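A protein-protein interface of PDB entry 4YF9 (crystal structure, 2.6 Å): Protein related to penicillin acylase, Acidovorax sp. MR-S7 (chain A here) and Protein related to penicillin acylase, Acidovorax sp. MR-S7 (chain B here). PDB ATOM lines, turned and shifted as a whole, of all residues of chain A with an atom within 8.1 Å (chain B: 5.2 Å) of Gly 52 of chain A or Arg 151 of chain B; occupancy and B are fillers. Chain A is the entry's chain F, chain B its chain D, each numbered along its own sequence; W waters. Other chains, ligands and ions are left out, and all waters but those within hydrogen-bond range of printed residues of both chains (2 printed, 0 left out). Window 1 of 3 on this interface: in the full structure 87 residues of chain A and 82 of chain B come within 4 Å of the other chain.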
ATOM      1  N   TRP A  24       4.703  -4.860 -11.098  1.00  0.00           N
ATOM      2  CA  TRP A  24       4.497  -5.391  -9.768  1.00  0.00           C
ATOM      3  C   TRP A  24       3.207  -6.134  -9.703  1.00  0.00           C
ATOM      4  O   TRP A  24       2.447  -6.145 -10.684  1.00  0.00           O
ATOM      5  CB  TRP A  24       4.502  -4.246  -8.771  1.00  0.00           C
ATOM      6  CG  TRP A  24       5.030  -4.612  -7.408  1.00  0.00           C
ATOM      7  CD1 TRP A  24       4.440  -4.360  -6.170  1.00  0.00           C
ATOM      8  CD2 TRP A  24       6.276  -5.312  -7.090  1.00  0.00           C
ATOM      9  NE1 TRP A  24       5.214  -4.838  -5.147  1.00  0.00           N
ATOM     10  CE2 TRP A  24       6.322  -5.423  -5.622  1.00  0.00           C
ATOM     11  CE3 TRP A  24       7.317  -5.836  -7.837  1.00  0.00           C
ATOM     12  CZ2 TRP A  24       7.373  -6.036  -4.967  1.00  0.00           C
ATOM     13  CZ3 TRP A  24       8.373  -6.454  -7.159  1.00  0.00           C
ATOM     14  CH2 TRP A  24       8.401  -6.546  -5.763  1.00  0.00           C
ATOM     15  N   GLY A  28      -2.668  -9.015  -3.747  1.00  0.00           N
ATOM     16  CA  GLY A  28      -1.824  -9.430  -2.632  1.00  0.00           C
ATOM     17  C   GLY A  28      -1.179  -8.287  -1.866  1.00  0.00           C
ATOM     18  O   GLY A  28      -1.275  -7.141  -2.280  1.00  0.00           O
ATOM     19  N   PRO A  29      -0.497  -8.597  -0.746  1.00  0.00           N
ATOM     20  CA  PRO A  29      -0.091  -7.549   0.211  1.00  0.00           C
ATOM     21  C   PRO A  29       1.061  -6.663  -0.258  1.00  0.00           C
ATOM     22  O   PRO A  29       1.291  -5.597   0.317  1.00  0.00           O
ATOM     23  CB  PRO A  29       0.308  -8.335   1.462  1.00  0.00           C
ATOM     24  CG  PRO A  29       0.597  -9.722   0.996  1.00  0.00           C
ATOM     25  CD  PRO A  29      -0.014  -9.937  -0.361  1.00  0.00           C
ATOM     26  N   ASP A  30       1.776  -7.095  -1.290  1.00  0.00           N
ATOM     27  CA  ASP A  30       2.838  -6.280  -1.866  1.00  0.00           C
ATOM     28  C   ASP A  30       2.335  -5.308  -2.943  1.00  0.00           C
ATOM     29  O   ASP A  30       3.119  -4.503  -3.438  1.00  0.00           O
ATOM     30  CB  ASP A  30       3.981  -7.164  -2.388  1.00  0.00           C
ATOM     31  CG  ASP A  30       4.749  -7.866  -1.260  1.00  0.00           C
ATOM     32  OD1 ASP A  30       4.391  -7.694  -0.074  1.00  0.00           O
ATOM     33  OD2 ASP A  30       5.717  -8.598  -1.554  1.00  0.00           O
ATOM     34  N   ARG A  31       1.040  -5.361  -3.290  1.00  0.00           N
ATOM     35  CA  ARG A  31       0.465  -4.413  -4.264  1.00  0.00           C
ATOM     36  C   ARG A  31       0.565  -2.985  -3.757  1.00  0.00           C
ATOM     37  O   ARG A  31       0.497  -2.726  -2.545  1.00  0.00           O
ATOM     38  CB  ARG A  31      -0.989  -4.743  -4.676  1.00  0.00           C
ATOM     39  CG  ARG A  31      -2.010  -4.789  -3.546  1.00  0.00           C
ATOM     40  CD  ARG A  31      -3.328  -4.061  -3.826  1.00  0.00           C
ATOM     41  NE  ARG A  31      -4.171  -4.739  -4.794  1.00  0.00           N
ATOM     42  CZ  ARG A  31      -5.445  -4.445  -5.045  1.00  0.00           C
ATOM     43  NH1 ARG A  31      -6.076  -3.480  -4.399  1.00  0.00           N
ATOM     44  NH2 ARG A  31      -6.089  -5.144  -5.961  1.00  0.00           N
ATOM     45  N   TYR A  33      -0.397   0.954  -3.075  1.00  0.00           N
ATOM     46  CA  TYR A  33      -1.547   1.724  -2.626  1.00  0.00           C
ATOM     47  C   TYR A  33      -1.186   3.202  -2.735  1.00  0.00           C
ATOM     48  O   TYR A  33      -0.169   3.641  -2.189  1.00  0.00           O
ATOM     49  CB  TYR A  33      -1.896   1.369  -1.186  1.00  0.00           C
ATOM     50  CG  TYR A  33      -3.121   2.078  -0.684  1.00  0.00           C
ATOM     51  CD1 TYR A  33      -4.394   1.538  -0.893  1.00  0.00           C
ATOM     52  CD2 TYR A  33      -3.020   3.294  -0.006  1.00  0.00           C
ATOM     53  CE1 TYR A  33      -5.529   2.186  -0.438  1.00  0.00           C
ATOM     54  CE2 TYR A  33      -4.156   3.951   0.453  1.00  0.00           C
ATOM     55  CZ  TYR A  33      -5.405   3.390   0.236  1.00  0.00           C
ATOM     56  OH  TYR A  33      -6.539   4.032   0.686  1.00  0.00           O
ATOM     57  N   SER A  49       2.646   3.056  -1.538  1.00  0.00           N
ATOM     58  CA  SER A  49       3.236   2.139  -0.566  1.00  0.00           C
ATOM     59  C   SER A  49       2.763   0.725  -0.861  1.00  0.00           C
ATOM     60  O   SER A  49       1.679   0.538  -1.430  1.00  0.00           O
ATOM     61  CB  SER A  49       2.765   2.500   0.850  1.00  0.00           C
ATOM     62  OG  SER A  49       3.224   3.778   1.250  1.00  0.00           O
ATOM     63  N   PHE A  50       3.555  -0.273  -0.467  1.00  0.00           N
ATOM     64  CA  PHE A  50       3.040  -1.636  -0.354  1.00  0.00           C
ATOM     65  C   PHE A  50       1.916  -1.535   0.669  1.00  0.00           C
ATOM     66  O   PHE A  50       2.002  -0.741   1.608  1.00  0.00           O
ATOM     67  CB  PHE A  50       4.081  -2.611   0.215  1.00  0.00           C
ATOM     68  CG  PHE A  50       5.232  -2.945  -0.704  1.00  0.00           C
ATOM     69  CD1 PHE A  50       5.245  -2.566  -2.048  1.00  0.00           C
ATOM     70  CD2 PHE A  50       6.301  -3.701  -0.215  1.00  0.00           C
ATOM     71  CE1 PHE A  50       6.316  -2.911  -2.866  1.00  0.00           C
ATOM     72  CE2 PHE A  50       7.373  -4.040  -1.035  1.00  0.00           C
ATOM     73  CZ  PHE A  50       7.379  -3.645  -2.360  1.00  0.00           C
ATOM     74  N   LEU A  51       0.864  -2.330   0.500  1.00  0.00           N
ATOM     75  CA  LEU A  51      -0.147  -2.446   1.539  1.00  0.00           C
ATOM     76  C   LEU A  51       0.554  -2.889   2.816  1.00  0.00           C
ATOM     77  O   LEU A  51       1.288  -3.888   2.810  1.00  0.00           O
ATOM     78  CB  LEU A  51      -1.207  -3.466   1.133  1.00  0.00           C
ATOM     79  CG  LEU A  51      -2.244  -3.085   0.075  1.00  0.00           C
ATOM     80  CD1 LEU A  51      -3.076  -4.311  -0.260  1.00  0.00           C
ATOM     81  CD2 LEU A  51      -3.138  -1.956   0.571  1.00  0.00           C
ATOM     82  N   GLY A  52       0.361  -2.142   3.899  1.00  0.00           N
ATOM     83  CA  GLY A  52       1.026  -2.461   5.159  1.00  0.00           C
ATOM     84  C   GLY A  52       2.204  -1.567   5.506  1.00  0.00           C
ATOM     85  O   GLY A  52       2.617  -1.517   6.669  1.00  0.00           O
ATOM     86  N   LEU A  53       2.739  -0.852   4.514  1.00  0.00           N
ATOM     87  CA  LEU A  53       3.833   0.108   4.741  1.00  0.00           C
ATOM     88  C   LEU A  53       3.333   1.530   4.993  1.00  0.00           C
ATOM     89  O   LEU A  53       2.425   1.993   4.298  1.00  0.00           O
ATOM     90  CB  LEU A  53       4.821   0.099   3.569  1.00  0.00           C
ATOM     91  CG  LEU A  53       5.700  -1.143   3.411  1.00  0.00           C
ATOM     92  CD1 LEU A  53       6.988  -0.794   2.690  1.00  0.00           C
ATOM     93  CD2 LEU A  53       6.043  -1.755   4.756  1.00  0.00           C
ATOM     94  N   PRO A  54       3.925   2.231   5.984  1.00  0.00           N
ATOM     95  CA  PRO A  54       3.423   3.545   6.385  1.00  0.00           C
ATOM     96  C   PRO A  54       4.058   4.769   5.709  1.00  0.00           C
ATOM     97  O   PRO A  54       3.523   5.866   5.846  1.00  0.00           O
ATOM     98  CB  PRO A  54       3.685   3.567   7.891  1.00  0.00           C
ATOM     99  CG  PRO A  54       4.884   2.712   8.068  1.00  0.00           C
ATOM    100  CD  PRO A  54       4.940   1.732   6.925  1.00  0.00           C
ATOM    101  N   VAL A  55       5.170   4.607   4.998  1.00  0.00           N
ATOM    102  CA  VAL A  55       5.744   5.742   4.265  1.00  0.00           C
ATOM    103  C   VAL A  55       5.793   5.464   2.769  1.00  0.00           C
ATOM    104  O   VAL A  55       5.697   4.315   2.348  1.00  0.00           O
ATOM    105  CB  VAL A  55       7.146   6.155   4.784  1.00  0.00           C
ATOM    106  CG1 VAL A  55       7.069   6.628   6.230  1.00  0.00           C
ATOM    107  CG2 VAL A  55       8.158   5.030   4.618  1.00  0.00           C
ATOM    108  N   GLN A  57       7.112   4.844  -0.894  1.00  0.00           N
ATOM    109  CA  GLN A  57       8.289   4.157  -1.422  1.00  0.00           C
ATOM    110  C   GLN A  57       8.673   4.651  -2.806  1.00  0.00           C
ATOM    111  O   GLN A  57       9.854   4.635  -3.178  1.00  0.00           O
ATOM    112  CB  GLN A  57       8.039   2.659  -1.472  1.00  0.00           C
ATOM    113  CG  GLN A  57       7.996   2.008  -0.107  1.00  0.00           C
ATOM    114  CD  GLN A  57       7.360   0.642  -0.171  1.00  0.00           C
ATOM    115  OE1 GLN A  57       6.158   0.500   0.037  1.00  0.00           O
ATOM    116  NE2 GLN A  57       8.157  -0.371  -0.477  1.00  0.00           N
ATOM    117  N   LEU A 162      13.303   1.883   6.136  1.00  0.00           N
ATOM    118  CA  LEU A 162      12.121   2.679   6.433  1.00  0.00           C
ATOM    119  C   LEU A 162      12.520   4.090   6.847  1.00  0.00           C
ATOM    120  O   LEU A 162      11.889   5.064   6.430  1.00  0.00           O
ATOM    121  CB  LEU A 162      11.294   1.988   7.523  1.00  0.00           C
ATOM    122  CG  LEU A 162       9.752   1.931   7.508  1.00  0.00           C
ATOM    123  CD1 LEU A 162       9.136   2.868   8.541  1.00  0.00           C
ATOM    124  CD2 LEU A 162       9.134   2.127   6.124  1.00  0.00           C
ATOM    125  N   GLN B  39      -6.010   2.366   4.261  1.00  0.00           N
ATOM    126  CA  GLN B  39      -5.497   1.135   3.658  1.00  0.00           C
ATOM    127  C   GLN B  39      -6.403  -0.046   3.975  1.00  0.00           C
ATOM    128  O   GLN B  39      -6.778  -0.815   3.084  1.00  0.00           O
ATOM    129  CB  GLN B  39      -4.063   0.850   4.108  1.00  0.00           C
ATOM    130  CG  GLN B  39      -3.014   1.661   3.364  1.00  0.00           C
ATOM    131  CD  GLN B  39      -1.600   1.172   3.622  1.00  0.00           C
ATOM    132  OE1 GLN B  39      -1.367  -0.024   3.807  1.00  0.00           O
ATOM    133  NE2 GLN B  39      -0.646   2.099   3.635  1.00  0.00           N
ATOM    134  N   MET B  47      -4.974  -7.348   3.350  1.00  0.00           N
ATOM    135  CA  MET B  47      -4.184  -6.977   4.525  1.00  0.00           C
ATOM    136  C   MET B  47      -4.318  -7.972   5.682  1.00  0.00           C
ATOM    137  O   MET B  47      -3.310  -8.404   6.245  1.00  0.00           O
ATOM    138  CB  MET B  47      -4.555  -5.564   4.993  1.00  0.00           C
ATOM    139  CG  MET B  47      -4.362  -4.472   3.944  1.00  0.00           C
ATOM    140  SD  MET B  47      -4.245  -2.816   4.652  1.00  0.00           S
ATOM    141  CE  MET B  47      -2.677  -2.914   5.512  1.00  0.00           C
ATOM    142  N   PHE B  51      -1.352 -10.274   7.428  1.00  0.00           N
ATOM    143  CA  PHE B  51      -0.828 -10.311   8.802  1.00  0.00           C
ATOM    144  C   PHE B  51      -0.763 -11.715   9.410  1.00  0.00           C
ATOM    145  O   PHE B  51       0.064 -11.983  10.273  1.00  0.00           O
ATOM    146  CB  PHE B  51      -1.530  -9.301   9.706  1.00  0.00           C
ATOM    147  CG  PHE B  51      -1.113  -7.890   9.436  1.00  0.00           C
ATOM    148  CD1 PHE B  51       0.106  -7.414   9.904  1.00  0.00           C
ATOM    149  CD2 PHE B  51      -1.912  -7.046   8.680  1.00  0.00           C
ATOM    150  CE1 PHE B  51       0.508  -6.116   9.639  1.00  0.00           C
ATOM    151  CE2 PHE B  51      -1.518  -5.750   8.412  1.00  0.00           C
ATOM    152  CZ  PHE B  51      -0.306  -5.282   8.889  1.00  0.00           C
ATOM    153  N   TYR B  54       2.772 -12.734   8.143  1.00  0.00           N
ATOM    154  CA  TYR B  54       3.958 -12.186   8.812  1.00  0.00           C
ATOM    155  C   TYR B  54       4.060 -12.615  10.264  1.00  0.00           C
ATOM    156  O   TYR B  54       5.161 -12.679  10.814  1.00  0.00           O
ATOM    157  CB  TYR B  54       4.042 -10.657   8.665  1.00  0.00           C
ATOM    158  CG  TYR B  54       3.774 -10.180   7.248  1.00  0.00           C
ATOM    159  CD1 TYR B  54       4.543 -10.632   6.181  1.00  0.00           C
ATOM    160  CD2 TYR B  54       2.731  -9.296   6.978  1.00  0.00           C
ATOM    161  CE1 TYR B  54       4.281 -10.217   4.885  1.00  0.00           C
ATOM    162  CE2 TYR B  54       2.462  -8.869   5.684  1.00  0.00           C
ATOM    163  CZ  TYR B  54       3.241  -9.330   4.641  1.00  0.00           C
ATOM    164  OH  TYR B  54       2.974  -8.910   3.354  1.00  0.00           O
ATOM    165  N   PHE B 113      -0.466   3.705  12.796  1.00  0.00           N
ATOM    166  CA  PHE B 113      -0.862   2.866  11.677  1.00  0.00           C
ATOM    167  C   PHE B 113      -1.634   1.647  12.175  1.00  0.00           C
ATOM    168  O   PHE B 113      -2.731   1.358  11.676  1.00  0.00           O
ATOM    169  CB  PHE B 113       0.369   2.450  10.862  1.00  0.00           C
ATOM    170  CG  PHE B 113       0.046   1.763   9.557  1.00  0.00           C
ATOM    171  CD1 PHE B 113      -0.250   0.399   9.519  1.00  0.00           C
ATOM    172  CD2 PHE B 113       0.062   2.474   8.360  1.00  0.00           C
ATOM    173  CE1 PHE B 113      -0.537  -0.234   8.316  1.00  0.00           C
ATOM    174  CE2 PHE B 113      -0.228   1.847   7.154  1.00  0.00           C
ATOM    175  CZ  PHE B 113      -0.528   0.492   7.131  1.00  0.00           C
ATOM    176  N   ASP B 147       3.489  -6.028  14.799  1.00  0.00           N
ATOM    177  CA  ASP B 147       3.044  -6.731  13.598  1.00  0.00           C
ATOM    178  C   ASP B 147       3.369  -5.938  12.335  1.00  0.00           C
ATOM    179  O   ASP B 147       3.785  -6.503  11.324  1.00  0.00           O
ATOM    180  CB  ASP B 147       1.548  -7.030  13.667  1.00  0.00           C
ATOM    181  CG  ASP B 147       1.205  -8.060  14.725  1.00  0.00           C
ATOM    182  OD1 ASP B 147       1.954  -9.049  14.879  1.00  0.00           O
ATOM    183  OD2 ASP B 147       0.173  -7.878  15.404  1.00  0.00           O
ATOM    184  N   VAL B 148       3.193  -4.621  12.404  1.00  0.00           N
ATOM    185  CA  VAL B 148       3.457  -3.763  11.255  1.00  0.00           C
ATOM    186  C   VAL B 148       4.961  -3.781  10.984  1.00  0.00           C
ATOM    187  O   VAL B 148       5.402  -3.817   9.827  1.00  0.00           O
ATOM    188  CB  VAL B 148       2.889  -2.341  11.456  1.00  0.00           C
ATOM    189  CG1 VAL B 148       3.169  -1.458  10.252  1.00  0.00           C
ATOM    190  CG2 VAL B 148       1.392  -2.400  11.703  1.00  0.00           C
ATOM    191  N   TRP B 149       5.735  -3.806  12.065  1.00  0.00           N
ATOM    192  CA  TRP B 149       7.181  -3.974  11.978  1.00  0.00           C
ATOM    193  C   TRP B 149       7.593  -5.296  11.388  1.00  0.00           C
ATOM    194  O   TRP B 149       8.530  -5.335  10.588  1.00  0.00           O
ATOM    195  CB  TRP B 149       7.844  -3.736  13.324  1.00  0.00           C
ATOM    196  CG  TRP B 149       7.935  -2.276  13.668  1.00  0.00           C
ATOM    197  CD1 TRP B 149       7.311  -1.611  14.712  1.00  0.00           C
ATOM    198  CD2 TRP B 149       8.688  -1.242  12.956  1.00  0.00           C
ATOM    199  NE1 TRP B 149       7.624  -0.276  14.703  1.00  0.00           N
ATOM    200  CE2 TRP B 149       8.446   0.011  13.678  1.00  0.00           C
ATOM    201  CE3 TRP B 149       9.521  -1.231  11.846  1.00  0.00           C
ATOM    202  CZ2 TRP B 149       9.021   1.209  13.285  1.00  0.00           C
ATOM    203  CZ3 TRP B 149      10.090  -0.011  11.451  1.00  0.00           C
ATOM    204  CH2 TRP B 149       9.841   1.178  12.156  1.00  0.00           C
ATOM    205  N   ARG B 150       6.907  -6.385  11.747  1.00  0.00           N
ATOM    206  CA  ARG B 150       7.107  -7.662  11.052  1.00  0.00           C
ATOM    207  C   ARG B 150       6.975  -7.474   9.536  1.00  0.00           C
ATOM    208  O   ARG B 150       7.827  -7.933   8.757  1.00  0.00           O
ATOM    209  CB  ARG B 150       6.089  -8.700  11.503  1.00  0.00           C
ATOM    210  CG  ARG B 150       6.332  -9.278  12.882  1.00  0.00           C
ATOM    211  CD  ARG B 150       5.220 -10.245  13.283  1.00  0.00           C
ATOM    212  NE  ARG B 150       5.623 -11.031  14.438  1.00  0.00           N
ATOM    213  CZ  ARG B 150       5.534 -10.623  15.700  1.00  0.00           C
ATOM    214  NH1 ARG B 150       5.036  -9.428  15.991  1.00  0.00           N
ATOM    215  NH2 ARG B 150       5.950 -11.417  16.678  1.00  0.00           N
ATOM    216  N   ARG B 151       5.913  -6.776   9.135  1.00  0.00           N
ATOM    217  CA  ARG B 151       5.586  -6.580   7.727  1.00  0.00           C
ATOM    218  C   ARG B 151       6.660  -5.758   7.029  1.00  0.00           C
ATOM    219  O   ARG B 151       7.036  -6.057   5.886  1.00  0.00           O
ATOM    220  CB  ARG B 151       4.223  -5.889   7.601  1.00  0.00           C
ATOM    221  CG  ARG B 151       3.630  -5.885   6.208  1.00  0.00           C
ATOM    222  CD  ARG B 151       4.029  -4.676   5.395  1.00  0.00           C
ATOM    223  NE  ARG B 151       3.652  -4.877   3.999  1.00  0.00           N
ATOM    224  CZ  ARG B 151       4.331  -5.625   3.127  1.00  0.00           C
ATOM    225  NH1 ARG B 151       5.437  -6.253   3.492  1.00  0.00           N
ATOM    226  NH2 ARG B 151       3.898  -5.746   1.881  1.00  0.00           N
ATOM    227  N   ILE B 152       7.135  -4.723   7.726  1.00  0.00           N
ATOM    228  CA  ILE B 152       8.182  -3.846   7.223  1.00  0.00           C
ATOM    229  C   ILE B 152       9.469  -4.656   7.048  1.00  0.00           C
ATOM    230  O   ILE B 152      10.128  -4.607   5.995  1.00  0.00           O
ATOM    231  CB  ILE B 152       8.392  -2.644   8.164  1.00  0.00           C
ATOM    232  CG1 ILE B 152       7.146  -1.756   8.146  1.00  0.00           C
ATOM    233  CG2 ILE B 152       9.602  -1.821   7.739  1.00  0.00           C
ATOM    234  CD1 ILE B 152       6.976  -0.884   9.367  1.00  0.00           C
ATOM    235  N   TYR B 153       9.792  -5.438   8.073  1.00  0.00           N
ATOM    236  CA  TYR B 153      10.969  -6.273   8.033  1.00  0.00           C
ATOM    237  C   TYR B 153      10.885  -7.284   6.897  1.00  0.00           C
ATOM    238  O   TYR B 153      11.874  -7.519   6.207  1.00  0.00           O
ATOM    239  CB  TYR B 153      11.192  -6.955   9.379  1.00  0.00           C
ATOM    240  CG  TYR B 153      12.517  -7.669   9.473  1.00  0.00           C
ATOM    241  CD1 TYR B 153      13.709  -6.962   9.463  1.00  0.00           C
ATOM    242  CD2 TYR B 153      12.572  -9.058   9.571  1.00  0.00           C
ATOM    243  CE1 TYR B 153      14.923  -7.616   9.549  1.00  0.00           C
ATOM    244  CE2 TYR B 153      13.782  -9.722   9.658  1.00  0.00           C
ATOM    245  CZ  TYR B 153      14.954  -8.995   9.645  1.00  0.00           C
ATOM    246  OH  TYR B 153      16.162  -9.646   9.729  1.00  0.00           O
ATOM    247  N   ALA B 154       9.702  -7.852   6.686  1.00  0.00           N
ATOM    248  CA  ALA B 154       9.482  -8.799   5.597  1.00  0.00           C
ATOM    249  C   ALA B 154       9.769  -8.211   4.211  1.00  0.00           C
ATOM    250  O   ALA B 154      10.293  -8.910   3.336  1.00  0.00           O
ATOM    251  CB  ALA B 154       8.071  -9.346   5.653  1.00  0.00           C
ATOM    252  N   ALA B 155       9.439  -6.933   4.022  1.00  0.00           N
ATOM    253  CA  ALA B 155       9.651  -6.253   2.737  1.00  0.00           C
ATOM    254  C   ALA B 155      11.124  -6.192   2.323  1.00  0.00           C
ATOM    255  O   ALA B 155      11.440  -6.182   1.128  1.00  0.00           O
ATOM    256  CB  ALA B 155       9.064  -4.853   2.772  1.00  0.00           C
HETATM  257  O   HOH W   1       6.997  -7.836   1.387  1.00  0.00           O
HETATM  258  O   HOH W   2       4.556 -10.085   1.512  1.00  0.00           O
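NH2 of Arg 151 of chain B lies within salt-bridge range of OD1 of Asp 30 of chain A (2.8 Å). The side-chain amide nitrogen of Gln 39 of chain B lies within hydrogen-bond range of the backbone carbonyl oxygen of Leu 53 of chain A (3.1 Å). The guanidinium group (NH2) of Arg 151 of chain B is in hydrogen-bond range of the backbone carbonyl oxygen (O) of Pro 29 of chain A (3.0 Å). OE1 of Gln 39 of chain B is in hydrogen-bond range of N of Gly 52 of chain A (2.7 Å). The guanidinium group of Arg 151 of chain B is in hydrogen-bond range of the backbone carbonyl oxygen of Leu 51 of chain A.
The backbone carbonyl oxygen (O) of Pro 29 of chain A is in hydrogen-bond range of the backbone NH (N) of Leu 51 of chain A (3.3 Å). The backbone NH (N) of Tyr 33 of chain A is in hydrogen-bond range of the backbone carbonyl oxygen (O) of Ser 49 of chain A (2.7 Å). The backbone carbonyl oxygen (O) of Arg 31 of chain A lies within hydrogen-bond range of the backbone NH (N) of Leu 51 of chain A, 3.1 Å away. The backbone carbonyl oxygen (O) of Asp 30 of chain A lies within hydrogen-bond range of the indole nitrogen (NE1) of Trp 24 of chain A, at 2.7 Å. N of Phe 50 of chain A lies within hydrogen-bond range of OE1 of Gln 57 of chain A, 2.8 Å away.
Asp 30 of chain A touches Tyr 54 of chain B. CB of Phe 50 of chain A touches NH2 of Arg 151 of chain B, 3.6 Å away. Gly 52 of chain A touches Met 47 of chain B. CZ of Phe 113 of chain B touches O of Gly 52 of chain A, 3.8 Å away. CG1 of Val 148 of chain B touches O of Gly 52 of chain A (3.6 Å). C of Gly 52 of chain A touches CD of Arg 151 of chain B, at 3.6 Å. Leu 53 of chain A touches Phe 113 of chain B. CD2 of Leu 53 of chain A touches CD of Arg 151 of chain B, at 3.6 Å. Phe 113 of chain B touches Pro 54 of chain A. Ile 152 of chain B touches Leu 162 of chain A (CG2 to CG, 3.8 Å).
Gly 52 of chain A touches five residues of chain B. Of the printed residues of chain A, Val 148 of chain B touches Gly 52. Printed residues of chain B within 4 Å of Phe 50 of chain A: Arg 151. Printed residues of chain A within 4 Å of Met 47 of chain B: Gly 52. Trp 24 of chain A touches none of the printed residues of chain B. Arg 150 of chain B touches none of the printed residues of chain A.
Printed residues of chain A that touch a printed residue of chain B: Pro 29, Asp 30, Tyr 33, Phe 50, Leu 51, Gly 52, Leu 53, Pro 54 and Leu 162. Hydrophobic or aromatic side chains of chain A within 4 Å of the printed part of chain B: Pro 29, Tyr 33, Phe 50, Leu 53, Pro 54 and Leu 162. Among the printed residues, 19 pairs touch across the chains.
Water W2 bridges the side-chain hydroxyl of Tyr 54 of chain B (2.7 Å) and the side-chain carboxylate of Asp 30 of chain A (2.9 Å). Water W1 bridges the side-chain carboxylate (OD1) of Asp 30 of chain A and the guanidinium group (NH1) of Arg 151 of chain B.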
